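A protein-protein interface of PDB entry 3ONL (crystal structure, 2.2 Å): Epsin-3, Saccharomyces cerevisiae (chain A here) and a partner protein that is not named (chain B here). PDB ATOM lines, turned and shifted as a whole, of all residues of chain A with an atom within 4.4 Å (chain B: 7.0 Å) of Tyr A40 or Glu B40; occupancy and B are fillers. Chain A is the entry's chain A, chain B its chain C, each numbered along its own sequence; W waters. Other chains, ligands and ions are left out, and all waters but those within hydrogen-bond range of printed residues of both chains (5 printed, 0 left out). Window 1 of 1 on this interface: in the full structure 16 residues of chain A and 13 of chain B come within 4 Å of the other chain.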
ATOM      1  N   SER A  36     -12.355  18.429 -22.853  1.00  0.00           N
ATOM      2  CA  SER A  36     -12.821  18.647 -21.488  1.00  0.00           C
ATOM      3  C   SER A  36     -11.901  17.999 -20.451  1.00  0.00           C
ATOM      4  O   SER A  36     -11.716  18.532 -19.354  1.00  0.00           O
ATOM      5  CB  SER A  36     -14.253  18.122 -21.324  1.00  0.00           C
ATOM      6  OG  SER A  36     -14.251  16.712 -21.131  1.00  0.00           O
ATOM      7  N   GLN A  37     -11.335  16.847 -20.807  1.00  0.00           N
ATOM      8  CA  GLN A  37     -10.383  16.152 -19.950  1.00  0.00           C
ATOM      9  C   GLN A  37      -9.125  16.992 -19.778  1.00  0.00           C
ATOM     10  O   GLN A  37      -8.518  16.995 -18.708  1.00  0.00           O
ATOM     11  CB  GLN A  37     -10.008  14.792 -20.540  1.00  0.00           C
ATOM     12  CG  GLN A  37     -11.137  13.761 -20.539  1.00  0.00           C
ATOM     13  CD  GLN A  37     -10.790  12.503 -21.321  1.00  0.00           C
ATOM     14  OE1 GLN A  37      -9.623  12.112 -21.420  1.00  0.00           O
ATOM     15  NE2 GLN A  37     -11.810  11.858 -21.880  1.00  0.00           N
ATOM     16  N   GLY A  38      -8.739  17.707 -20.833  1.00  0.00           N
ATOM     17  CA  GLY A  38      -7.542  18.552 -20.786  1.00  0.00           C
ATOM     18  C   GLY A  38      -7.641  19.672 -19.766  1.00  0.00           C
ATOM     19  O   GLY A  38      -6.625  20.163 -19.278  1.00  0.00           O
ATOM     20  N   THR A  39      -8.866  20.082 -19.425  1.00  0.00           N
ATOM     21  CA  THR A  39      -9.048  21.172 -18.470  1.00  0.00           C
ATOM     22  C   THR A  39      -8.662  20.803 -17.025  1.00  0.00           C
ATOM     23  O   THR A  39      -8.662  21.671 -16.152  1.00  0.00           O
ATOM     24  CB  THR A  39     -10.477  21.728 -18.489  1.00  0.00           C
ATOM     25  OG1 THR A  39     -11.367  20.753 -17.935  1.00  0.00           O
ATOM     26  CG2 THR A  39     -10.914  22.096 -19.929  1.00  0.00           C
ATOM     27  N   TYR A  40      -8.333  19.531 -16.779  1.00  0.00           N
ATOM     28  CA  TYR A  40      -7.955  19.064 -15.427  1.00  0.00           C
ATOM     29  C   TYR A  40      -6.452  19.053 -15.119  1.00  0.00           C
ATOM     30  O   TYR A  40      -6.032  18.511 -14.085  1.00  0.00           O
ATOM     31  CB  TYR A  40      -8.591  17.698 -15.108  1.00  0.00           C
ATOM     32  CG  TYR A  40     -10.082  17.797 -14.920  1.00  0.00           C
ATOM     33  CD1 TYR A  40     -10.644  17.956 -13.650  1.00  0.00           C
ATOM     34  CD2 TYR A  40     -10.935  17.769 -16.026  1.00  0.00           C
ATOM     35  CE1 TYR A  40     -12.020  18.076 -13.493  1.00  0.00           C
ATOM     36  CE2 TYR A  40     -12.289  17.886 -15.883  1.00  0.00           C
ATOM     37  CZ  TYR A  40     -12.832  18.038 -14.625  1.00  0.00           C
ATOM     38  OH  TYR A  40     -14.192  18.133 -14.527  1.00  0.00           O
ATOM     39  N   ASN A  41      -5.654  19.635 -16.015  1.00  0.00           N
ATOM     40  CA  ASN A  41      -4.247  19.955 -15.724  1.00  0.00           C
ATOM     41  C   ASN A  41      -3.883  21.332 -16.254  1.00  0.00           C
ATOM     42  O   ASN A  41      -4.398  21.760 -17.291  1.00  0.00           O
ATOM     43  CB  ASN A  41      -3.274  18.897 -16.264  1.00  0.00           C
ATOM     44  CG  ASN A  41      -3.302  18.789 -17.788  1.00  0.00           C
ATOM     45  OD1 ASN A  41      -4.088  18.032 -18.355  1.00  0.00           O
ATOM     46  ND2 ASN A  41      -2.433  19.536 -18.448  1.00  0.00           N
ATOM     47  N   HIS A  80     -18.811  20.231 -18.796  1.00  0.00           N
ATOM     48  CA  HIS A  80     -18.043  18.989 -18.664  1.00  0.00           C
ATOM     49  C   HIS A  80     -16.600  19.172 -18.182  1.00  0.00           C
ATOM     50  O   HIS A  80     -15.930  18.183 -17.903  1.00  0.00           O
ATOM     51  CB  HIS A  80     -18.020  18.200 -19.987  1.00  0.00           C
ATOM     52  CG  HIS A  80     -19.371  17.874 -20.544  1.00  0.00           C
ATOM     53  ND1 HIS A  80     -19.975  16.647 -20.363  1.00  0.00           N
ATOM     54  CD2 HIS A  80     -20.218  18.598 -21.315  1.00  0.00           C
ATOM     55  CE1 HIS A  80     -21.145  16.639 -20.980  1.00  0.00           C
ATOM     56  NE2 HIS A  80     -21.315  17.810 -21.568  1.00  0.00           N
ATOM     57  N   GLY A  81     -16.109  20.414 -18.119  1.00  0.00           N
ATOM     58  CA  GLY A  81     -14.713  20.670 -17.736  1.00  0.00           C
ATOM     59  C   GLY A  81     -14.528  20.969 -16.254  1.00  0.00           C
ATOM     60  O   GLY A  81     -15.481  20.932 -15.483  1.00  0.00           O
ATOM     61  N   SER A  82     -13.296  21.264 -15.852  1.00  0.00           N
ATOM     62  CA  SER A  82     -12.997  21.563 -14.451  1.00  0.00           C
ATOM     63  C   SER A  82     -13.618  22.876 -13.960  1.00  0.00           C
ATOM     64  O   SER A  82     -13.788  23.816 -14.725  1.00  0.00           O
ATOM     65  CB  SER A  82     -11.492  21.607 -14.231  1.00  0.00           C
ATOM     66  OG  SER A  82     -10.899  22.635 -15.009  1.00  0.00           O
ATOM     67  N   GLU A  83     -13.950  22.923 -12.673  1.00  0.00           N
ATOM     68  CA  GLU A  83     -14.356  24.168 -12.015  1.00  0.00           C
ATOM     69  C   GLU A  83     -13.341  25.297 -12.237  1.00  0.00           C
ATOM     70  O   GLU A  83     -13.727  26.438 -12.487  1.00  0.00           O
ATOM     71  CB  GLU A  83     -14.583  23.937 -10.519  1.00  0.00           C
ATOM     72  CG  GLU A  83     -15.876  23.189 -10.202  1.00  0.00           C
ATOM     73  CD  GLU A  83     -16.057  22.912  -8.713  1.00  0.00           C
ATOM     74  OE1 GLU A  83     -15.249  23.408  -7.893  1.00  0.00           O
ATOM     75  OE2 GLU A  83     -17.019  22.192  -8.362  1.00  0.00           O
ATOM     76  N   ARG A 137     -24.332  21.129 -14.915  1.00  0.00           N
ATOM     77  CA  ARG A 137     -23.305  20.099 -14.691  1.00  0.00           C
ATOM     78  C   ARG A 137     -23.918  18.780 -14.199  1.00  0.00           C
ATOM     79  O   ARG A 137     -23.499  17.700 -14.629  1.00  0.00           O
ATOM     80  CB  ARG A 137     -22.213  20.600 -13.739  1.00  0.00           C
ATOM     81  CG  ARG A 137     -21.437  21.822 -14.257  1.00  0.00           C
ATOM     82  CD  ARG A 137     -20.359  22.251 -13.275  1.00  0.00           C
ATOM     83  NE  ARG A 137     -19.050  21.708 -13.622  1.00  0.00           N
ATOM     84  CZ  ARG A 137     -18.169  21.225 -12.751  1.00  0.00           C
ATOM     85  NH1 ARG A 137     -18.446  21.172 -11.448  1.00  0.00           N
ATOM     86  NH2 ARG A 137     -17.007  20.768 -13.190  1.00  0.00           N
ATOM     87  N   ARG A 141     -23.855  15.061 -16.329  1.00  0.00           N
ATOM     88  CA  ARG A 141     -23.418  13.789 -15.750  1.00  0.00           C
ATOM     89  C   ARG A 141     -24.422  12.656 -15.971  1.00  0.00           C
ATOM     90  O   ARG A 141     -24.044  11.568 -16.422  1.00  0.00           O
ATOM     91  CB  ARG A 141     -23.092  13.965 -14.263  1.00  0.00           C
ATOM     92  CG  ARG A 141     -21.738  14.618 -14.042  1.00  0.00           C
ATOM     93  CD  ARG A 141     -21.696  15.484 -12.792  1.00  0.00           C
ATOM     94  NE  ARG A 141     -20.392  16.140 -12.681  1.00  0.00           N
ATOM     95  CZ  ARG A 141     -20.044  16.975 -11.706  1.00  0.00           C
ATOM     96  NH1 ARG A 141     -20.904  17.272 -10.735  1.00  0.00           N
ATOM     97  NH2 ARG A 141     -18.827  17.514 -11.698  1.00  0.00           N
ATOM     98  N   ALA B  17     -12.926   8.588  -3.215  1.00  0.00           N
ATOM     99  CA  ALA B  17     -12.342   9.832  -3.689  1.00  0.00           C
ATOM    100  C   ALA B  17     -10.951  10.011  -3.084  1.00  0.00           C
ATOM    101  O   ALA B  17     -10.017  10.406  -3.777  1.00  0.00           O
ATOM    102  CB  ALA B  17     -13.263  11.022  -3.351  1.00  0.00           C
ATOM    103  N   LEU B  29      -0.526  11.479 -17.205  1.00  0.00           N
ATOM    104  CA  LEU B  29      -1.419  12.619 -17.423  1.00  0.00           C
ATOM    105  C   LEU B  29      -2.789  12.264 -18.025  1.00  0.00           C
ATOM    106  O   LEU B  29      -3.824  12.720 -17.532  1.00  0.00           O
ATOM    107  CB  LEU B  29      -0.701  13.664 -18.294  1.00  0.00           C
ATOM    108  CG  LEU B  29      -1.163  15.131 -18.378  1.00  0.00           C
ATOM    109  CD1 LEU B  29      -2.310  15.313 -19.376  1.00  0.00           C
ATOM    110  CD2 LEU B  29      -1.531  15.694 -17.010  1.00  0.00           C
ATOM    111  N   ARG B  32      -4.607  10.543 -15.464  1.00  0.00           N
ATOM    112  CA  ARG B  32      -4.764  11.443 -14.324  1.00  0.00           C
ATOM    113  C   ARG B  32      -5.921  12.432 -14.497  1.00  0.00           C
ATOM    114  O   ARG B  32      -6.633  12.702 -13.533  1.00  0.00           O
ATOM    115  CB  ARG B  32      -3.475  12.200 -14.050  1.00  0.00           C
ATOM    116  CG  ARG B  32      -3.398  12.789 -12.643  1.00  0.00           C
ATOM    117  CD  ARG B  32      -2.185  13.662 -12.502  1.00  0.00           C
ATOM    118  NE  ARG B  32      -0.957  12.922 -12.791  1.00  0.00           N
ATOM    119  CZ  ARG B  32       0.133  13.464 -13.325  1.00  0.00           C
ATOM    120  NH1 ARG B  32       0.156  14.754 -13.641  1.00  0.00           N
ATOM    121  NH2 ARG B  32       1.196  12.711 -13.555  1.00  0.00           N
ATOM    122  N   ASN B  33      -6.097  12.960 -15.714  1.00  0.00           N
ATOM    123  CA  ASN B  33      -7.235  13.819 -16.046  1.00  0.00           C
ATOM    124  C   ASN B  33      -8.578  13.165 -15.753  1.00  0.00           C
ATOM    125  O   ASN B  33      -9.456  13.785 -15.160  1.00  0.00           O
ATOM    126  CB  ASN B  33      -7.231  14.207 -17.531  1.00  0.00           C
ATOM    127  CG  ASN B  33      -6.007  15.012 -17.935  1.00  0.00           C
ATOM    128  OD1 ASN B  33      -5.487  14.835 -19.038  1.00  0.00           O
ATOM    129  ND2 ASN B  33      -5.544  15.897 -17.053  1.00  0.00           N
ATOM    130  N   THR B  34      -8.734  11.927 -16.209  1.00  0.00           N
ATOM    131  CA  THR B  34      -9.964  11.174 -16.024  1.00  0.00           C
ATOM    132  C   THR B  34     -10.212  10.983 -14.534  1.00  0.00           C
ATOM    133  O   THR B  34     -11.334  11.177 -14.054  1.00  0.00           O
ATOM    134  CB  THR B  34      -9.893   9.803 -16.748  1.00  0.00           C
ATOM    135  OG1 THR B  34      -9.697  10.016 -18.149  1.00  0.00           O
ATOM    136  CG2 THR B  34     -11.181   9.013 -16.551  1.00  0.00           C
ATOM    137  N   THR B  35      -9.150  10.642 -13.808  1.00  0.00           N
ATOM    138  CA  THR B  35      -9.236  10.398 -12.370  1.00  0.00           C
ATOM    139  C   THR B  35      -9.688  11.654 -11.618  1.00  0.00           C
ATOM    140  O   THR B  35     -10.656  11.603 -10.860  1.00  0.00           O
ATOM    141  CB  THR B  35      -7.902   9.856 -11.814  1.00  0.00           C
ATOM    142  OG1 THR B  35      -7.570   8.657 -12.511  1.00  0.00           O
ATOM    143  CG2 THR B  35      -8.010   9.533 -10.326  1.00  0.00           C
ATOM    144  N   LEU B  36      -9.017  12.780 -11.860  1.00  0.00           N
ATOM    145  CA  LEU B  36      -9.408  14.049 -11.228  1.00  0.00           C
ATOM    146  C   LEU B  36     -10.831  14.480 -11.606  1.00  0.00           C
ATOM    147  O   LEU B  36     -11.597  14.944 -10.755  1.00  0.00           O
ATOM    148  CB  LEU B  36      -8.386  15.155 -11.524  1.00  0.00           C
ATOM    149  CG  LEU B  36      -6.963  14.910 -10.987  1.00  0.00           C
ATOM    150  CD1 LEU B  36      -6.057  16.138 -11.188  1.00  0.00           C
ATOM    151  CD2 LEU B  36      -6.952  14.503  -9.517  1.00  0.00           C
ATOM    152  N   LYS B  37     -11.205  14.301 -12.869  1.00  0.00           N
ATOM    153  CA  LYS B  37     -12.569  14.620 -13.273  1.00  0.00           C
ATOM    154  C   LYS B  37     -13.601  13.785 -12.504  1.00  0.00           C
ATOM    155  O   LYS B  37     -14.630  14.307 -12.081  1.00  0.00           O
ATOM    156  CB  LYS B  37     -12.760  14.470 -14.779  1.00  0.00           C
ATOM    157  CG  LYS B  37     -14.172  14.806 -15.231  1.00  0.00           C
ATOM    158  CD  LYS B  37     -14.338  14.651 -16.742  1.00  0.00           C
ATOM    159  CE  LYS B  37     -15.727  15.098 -17.163  1.00  0.00           C
ATOM    160  NZ  LYS B  37     -15.947  14.936 -18.632  1.00  0.00           N
ATOM    161  N   HIS B  38     -13.323  12.501 -12.309  1.00  0.00           N
ATOM    162  CA  HIS B  38     -14.202  11.671 -11.498  1.00  0.00           C
ATOM    163  C   HIS B  38     -14.234  12.100 -10.025  1.00  0.00           C
ATOM    164  O   HIS B  38     -15.296  12.089  -9.402  1.00  0.00           O
ATOM    165  CB  HIS B  38     -13.841  10.192 -11.609  1.00  0.00           C
ATOM    166  CG  HIS B  38     -14.848   9.290 -10.967  1.00  0.00           C
ATOM    167  ND1 HIS B  38     -14.557   8.512  -9.868  1.00  0.00           N
ATOM    168  CD2 HIS B  38     -16.157   9.077 -11.245  1.00  0.00           C
ATOM    169  CE1 HIS B  38     -15.638   7.840  -9.510  1.00  0.00           C
ATOM    170  NE2 HIS B  38     -16.623   8.168 -10.327  1.00  0.00           N
ATOM    171  N   VAL B  39     -13.079  12.472  -9.472  1.00  0.00           N
ATOM    172  CA  VAL B  39     -13.020  12.960  -8.089  1.00  0.00           C
ATOM    173  C   VAL B  39     -13.853  14.237  -7.938  1.00  0.00           C
ATOM    174  O   VAL B  39     -14.542  14.423  -6.934  1.00  0.00           O
ATOM    175  CB  VAL B  39     -11.567  13.222  -7.622  1.00  0.00           C
ATOM    176  CG1 VAL B  39     -11.554  13.748  -6.207  1.00  0.00           C
ATOM    177  CG2 VAL B  39     -10.756  11.943  -7.681  1.00  0.00           C
ATOM    178  N   GLU B  40     -13.819  15.097  -8.950  1.00  0.00           N
ATOM    179  CA  GLU B  40     -14.588  16.340  -8.905  1.00  0.00           C
ATOM    180  C   GLU B  40     -16.085  16.055  -8.869  1.00  0.00           C
ATOM    181  O   GLU B  40     -16.842  16.719  -8.159  1.00  0.00           O
ATOM    182  CB  GLU B  40     -14.237  17.252 -10.088  1.00  0.00           C
ATOM    183  CG  GLU B  40     -14.846  18.670  -9.983  1.00  0.00           C
ATOM    184  CD  GLU B  40     -14.561  19.488 -11.221  1.00  0.00           C
ATOM    185  OE1 GLU B  40     -15.096  19.129 -12.290  1.00  0.00           O
ATOM    186  OE2 GLU B  40     -13.789  20.470 -11.135  1.00  0.00           O
ATOM    187  N   GLN B  41     -16.504  15.050  -9.627  1.00  0.00           N
ATOM    188  CA  GLN B  41     -17.882  14.590  -9.608  1.00  0.00           C
ATOM    189  C   GLN B  41     -18.228  14.021  -8.224  1.00  0.00           C
ATOM    190  O   GLN B  41     -19.292  14.304  -7.676  1.00  0.00           O
ATOM    191  CB  GLN B  41     -18.091  13.529 -10.696  1.00  0.00           C
ATOM    192  CG  GLN B  41     -19.484  12.905 -10.710  1.00  0.00           C
ATOM    193  CD  GLN B  41     -19.662  11.874 -11.821  1.00  0.00           C
ATOM    194  OE1 GLN B  41     -20.055  10.736 -11.568  1.00  0.00           O
ATOM    195  NE2 GLN B  41     -19.365  12.270 -13.054  1.00  0.00           N
ATOM    196  N   GLN B  42     -17.317  13.241  -7.652  1.00  0.00           N
ATOM    197  CA  GLN B  42     -17.556  12.656  -6.332  1.00  0.00           C
ATOM    198  C   GLN B  42     -17.647  13.716  -5.244  1.00  0.00           C
ATOM    199  O   GLN B  42     -18.473  13.601  -4.329  1.00  0.00           O
ATOM    200  CB  GLN B  42     -16.494  11.613  -5.993  1.00  0.00           C
ATOM    201  CG  GLN B  42     -16.612  10.370  -6.863  1.00  0.00           C
ATOM    202  CD  GLN B  42     -15.879   9.187  -6.294  1.00  0.00           C
ATOM    203  OE1 GLN B  42     -14.704   9.283  -5.916  1.00  0.00           O
ATOM    204  NE2 GLN B  42     -16.568   8.056  -6.222  1.00  0.00           N
ATOM    205  N   GLN B  43     -16.813  14.752  -5.357  1.00  0.00           N
ATOM    206  CA  GLN B  43     -16.881  15.924  -4.467  1.00  0.00           C
ATOM    207  C   GLN B  43     -18.292  16.534  -4.468  1.00  0.00           C
ATOM    208  O   GLN B  43     -18.881  16.777  -3.414  1.00  0.00           O
ATOM    209  CB  GLN B  43     -15.840  16.966  -4.901  1.00  0.00           C
ATOM    210  CG  GLN B  43     -15.949  18.337  -4.239  1.00  0.00           C
ATOM    211  CD  GLN B  43     -15.161  19.394  -4.997  1.00  0.00           C
ATOM    212  OE1 GLN B  43     -15.724  20.184  -5.755  1.00  0.00           O
ATOM    213  NE2 GLN B  43     -13.849  19.388  -4.823  1.00  0.00           N
ATOM    214  N   ASP B  44     -18.825  16.784  -5.659  1.00  0.00           N
ATOM    215  CA  ASP B  44     -20.200  17.259  -5.794  1.00  0.00           C
ATOM    216  C   ASP B  44     -21.201  16.260  -5.216  1.00  0.00           C
ATOM    217  O   ASP B  44     -22.167  16.655  -4.580  1.00  0.00           O
ATOM    218  CB  ASP B  44     -20.537  17.540  -7.265  1.00  0.00           C
ATOM    219  CG  ASP B  44     -19.747  18.716  -7.845  1.00  0.00           C
ATOM    220  OD1 ASP B  44     -19.097  19.472  -7.085  1.00  0.00           O
ATOM    221  OD2 ASP B  44     -19.785  18.885  -9.084  1.00  0.00           O
ATOM    222  N   GLU B  45     -20.974  14.963  -5.428  1.00  0.00           N
ATOM    223  CA  GLU B  45     -21.887  13.953  -4.892  1.00  0.00           C
ATOM    224  C   GLU B  45     -21.902  13.999  -3.361  1.00  0.00           C
ATOM    225  O   GLU B  45     -22.951  13.851  -2.740  1.00  0.00           O
ATOM    226  CB  GLU B  45     -21.530  12.535  -5.389  1.00  0.00           C
ATOM    227  CG  GLU B  45     -21.792  12.305  -6.883  1.00  0.00           C
ATOM    228  CD  GLU B  45     -21.370  10.923  -7.361  1.00  0.00           C
ATOM    229  OE1 GLU B  45     -20.727  10.173  -6.589  1.00  0.00           O
ATOM    230  OE2 GLU B  45     -21.685  10.581  -8.520  1.00  0.00           O
ATOM    231  N   ILE B  85     -10.868  16.441   0.336  1.00  0.00           N
ATOM    232  CA  ILE B  85     -11.261  16.245  -1.062  1.00  0.00           C
ATOM    233  C   ILE B  85     -11.058  17.510  -1.890  1.00  0.00           C
ATOM    234  O   ILE B  85     -10.208  17.541  -2.782  1.00  0.00           O
ATOM    235  CB  ILE B  85     -12.731  15.747  -1.226  1.00  0.00           C
ATOM    236  CG1 ILE B  85     -12.987  14.458  -0.427  1.00  0.00           C
ATOM    237  CG2 ILE B  85     -13.076  15.538  -2.731  1.00  0.00           C
ATOM    238  CD1 ILE B  85     -12.114  13.287  -0.831  1.00  0.00           C
ATOM    239  N   LEU B  89      -7.858  18.262  -4.375  1.00  0.00           N
ATOM    240  CA  LEU B  89      -8.266  18.193  -5.781  1.00  0.00           C
ATOM    241  C   LEU B  89      -7.942  19.492  -6.519  1.00  0.00           C
ATOM    242  O   LEU B  89      -7.347  19.467  -7.599  1.00  0.00           O
ATOM    243  CB  LEU B  89      -9.755  17.866  -5.926  1.00  0.00           C
ATOM    244  CG  LEU B  89     -10.337  18.020  -7.341  1.00  0.00           C
ATOM    245  CD1 LEU B  89      -9.723  17.014  -8.313  1.00  0.00           C
ATOM    246  CD2 LEU B  89     -11.851  17.898  -7.338  1.00  0.00           C
ATOM    247  N   GLN B  90      -8.330  20.617  -5.924  1.00  0.00           N
ATOM    248  CA  GLN B  90      -8.059  21.932  -6.501  1.00  0.00           C
ATOM    249  C   GLN B  90      -6.558  22.097  -6.716  1.00  0.00           C
ATOM    250  O   GLN B  90      -6.117  22.538  -7.774  1.00  0.00           O
ATOM    251  CB  GLN B  90      -8.580  23.034  -5.576  1.00  0.00           C
ATOM    252  CG  GLN B  90      -9.420  24.101  -6.265  1.00  0.00           C
ATOM    253  CD  GLN B  90     -10.901  23.754  -6.308  1.00  0.00           C
ATOM    254  OE1 GLN B  90     -11.737  24.504  -5.783  1.00  0.00           O
ATOM    255  NE2 GLN B  90     -11.233  22.612  -6.931  1.00  0.00           N
ATOM    256  N   LEU B  92      -4.264  19.747  -7.134  1.00  0.00           N
ATOM    257  CA  LEU B  92      -3.844  18.893  -8.250  1.00  0.00           C
ATOM    258  C   LEU B  92      -4.235  19.456  -9.616  1.00  0.00           C
ATOM    259  O   LEU B  92      -3.452  19.411 -10.561  1.00  0.00           O
ATOM    260  CB  LEU B  92      -4.414  17.487  -8.074  1.00  0.00           C
ATOM    261  CG  LEU B  92      -3.515  16.355  -7.567  1.00  0.00           C
ATOM    262  CD1 LEU B  92      -2.250  16.842  -6.858  1.00  0.00           C
ATOM    263  CD2 LEU B  92      -4.315  15.408  -6.691  1.00  0.00           C
ATOM    264  N   VAL B  93      -5.451  19.985  -9.719  1.00  0.00           N
ATOM    265  CA  VAL B  93      -5.916  20.569 -10.969  1.00  0.00           C
ATOM    266  C   VAL B  93      -5.132  21.861 -11.258  1.00  0.00           C
ATOM    267  O   VAL B  93      -4.919  22.224 -12.411  1.00  0.00           O
ATOM    268  CB  VAL B  93      -7.464  20.771 -10.975  1.00  0.00           C
ATOM    269  CG1 VAL B  93      -7.927  21.582 -12.185  1.00  0.00           C
ATOM    270  CG2 VAL B  93      -8.187  19.414 -10.963  1.00  0.00           C
ATOM    271  N   ASP B  94      -4.664  22.528 -10.207  1.00  0.00           N
ATOM    272  CA  ASP B  94      -3.876  23.745 -10.374  1.00  0.00           C
ATOM    273  C   ASP B  94      -2.399  23.513 -10.705  1.00  0.00           C
ATOM    274  O   ASP B  94      -1.794  24.341 -11.382  1.00  0.00           O
ATOM    275  CB  ASP B  94      -4.044  24.673  -9.169  1.00  0.00           C
ATOM    276  CG  ASP B  94      -5.410  25.335  -9.137  1.00  0.00           C
ATOM    277  OD1 ASP B  94      -5.682  26.098  -8.190  1.00  0.00           O
ATOM    278  OD2 ASP B  94      -6.218  25.088 -10.060  1.00  0.00           O
ATOM    279  N   SER B  95      -1.827  22.404 -10.234  1.00  0.00           N
ATOM    280  CA  SER B  95      -0.484  21.961 -10.651  1.00  0.00           C
ATOM    281  C   SER B  95      -0.233  20.491 -10.313  1.00  0.00           C
ATOM    282  O   SER B  95       0.793  19.917 -10.715  1.00  0.00           O
ATOM    283  CB  SER B  95       0.619  22.829 -10.038  1.00  0.00           C
ATOM    284  OG  SER B  95       0.757  24.053 -10.736  1.00  0.00           O
HETATM  285  O   HOH W   1      -4.591  16.168 -14.469  1.00  0.00           O
HETATM  286  O   HOH W   2     -13.703  21.493  -6.955  1.00  0.00           O
HETATM  287  O   HOH W   3     -18.828  15.392 -18.150  1.00  0.00           O
HETATM  288  O   HOH W   4      -6.929  12.507 -20.560  1.00  0.00           O
HETATM  289  O   HOH W   5     -16.560  16.223 -12.996  1.00  0.00           O
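Of chain B, only Asn B33 (3.8 Å), Leu B36 (3.7 Å), Lys B37 (3.4 Å), Glu B40 (2.6 Å) and Val B93 (3.7 Å) come within 4 Å of Tyr A40.
Printed residues of chain A within 4 Å of Thr B34: Gln A37.
Of the printed residues of chain A, Glu B40 touches Tyr A40, Gly A81, Ser A82, Glu A83 and Arg A137.
Of the printed residues of chain A, Gln B41 touches Arg A141.
Printed residues of chain A within 4 Å of Asp B44: Glu A83, Arg A137 and Arg A141.
The nearest residue of chain A that does not touch Glu B40 is Arg A141 (4.1 Å).
The nearest printed residue of chain B that does not touch Gln A37 is Lys B37 (5.0 Å).
Among the printed residues, merely in contact across the chains: Gln A37 with Asn B33, Tyr A40 with Lys B37, Asn A41 with Leu B29, Arg A141 with Gln B41, Ser A36 with Lys B37, Glu A83 with Gln B43, Ser A82 with Glu B40, Glu A83 with Asp B44, Gly A81 with Glu B40, Tyr A40 with Val B93, Tyr A40 with Leu B36, Tyr A40 with Asn B33 and Gln A37 with Thr B34.
The backbone carbonyl oxygen (O) of Ser A36 sits at hydrogen-bond distance from the side-chain hydroxyl (OG1) of Thr A39 (2.7 Å).
OD1 of Asn A41 sits close to O of Gly A38 (3.4 Å).
OG of Ser A82 sits at hydrogen-bond distance from O of Thr A39.
The guanidinium group of Arg A137 is in hydrogen-bond range of the backbone carbonyl oxygen of Gly A81, at 2.8 Å.
The guanidinium group of Arg A137 is in salt-bridge range of the side-chain carboxylate of Glu A83 (3.5 Å).
The side-chain amide oxygen (OE1) of Gln B41 sits close to the side-chain carboxylate (OE2) of Glu B45, 3.5 Å away.
The side-chain carboxylate of Glu B40 lies within hydrogen-bond range of the side-chain hydroxyl of Tyr A40, 2.6 Å away.
OD1 of Asn A41 lies within hydrogen-bond range of ND2 of Asn B33.
The backbone carbonyl oxygen (O) of His A80 sits close to the side-chain amino group (NZ) of Lys B37, at 3.3 Å.
The backbone NH (N) of Glu A83 sits at hydrogen-bond distance from the side-chain carboxylate (OE2) of Glu B40 (2.9 Å).
OE1 of Glu B40 lies within salt-bridge range of NH2 of Arg A137, at 2.7 Å.
The guanidinium group (NH1) of Arg A137 lies within salt-bridge range of the side-chain carboxylate (OD2) of Asp B44, 3.6 Å away.
The guanidinium group of Arg A141 is in salt-bridge range of the side-chain carboxylate of Asp B44.
Of the 12 printed residues of chain A, 10 touch a printed residue of chain B.
Hydrophobic or aromatic side chains of chain A within 4 Å of the printed part of chain B: Tyr A40.
Of the 23 printed residues of chain B, 10 touch a printed residue of chain A.
Among the printed residues, 20 pairs touch across the chains.
Among the printed residues, Asp or Glu carboxylates within 4 Å of a Lys or Arg side-chain nitrogen of the other chain: Arg A137 with Glu B40 (2.7 Å), Arg A137 with Asp B44 (3.6 Å) and Arg A141 with Asp B44 (2.6 Å).
Water W2 lies within hydrogen-bond range of OE1 of Glu A83 (2.6 Å), OE1 of Gln B43 (2.7 Å) and NE2 of Gln B90 (2.7 Å).
Water W1 bridges the side-chain amide nitrogen of Asn B33 and the backbone carbonyl oxygen of Tyr A40.
Water W3 lies within hydrogen-bond range of ND1 of His A80 (2.8 Å) and NZ of Lys B37 (3.0 Å).
Water W4 bridges the side-chain amide oxygen of Gln A37 and the side-chain amide oxygen of Asn B33.
Water W5 lies within hydrogen-bond range of O of Lys B37 (2.9 Å), NH2 of Arg A141 (2.9 Å), OE1 of Glu B40 (3.3 Å) and OH of Tyr A40 (3.4 Å).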
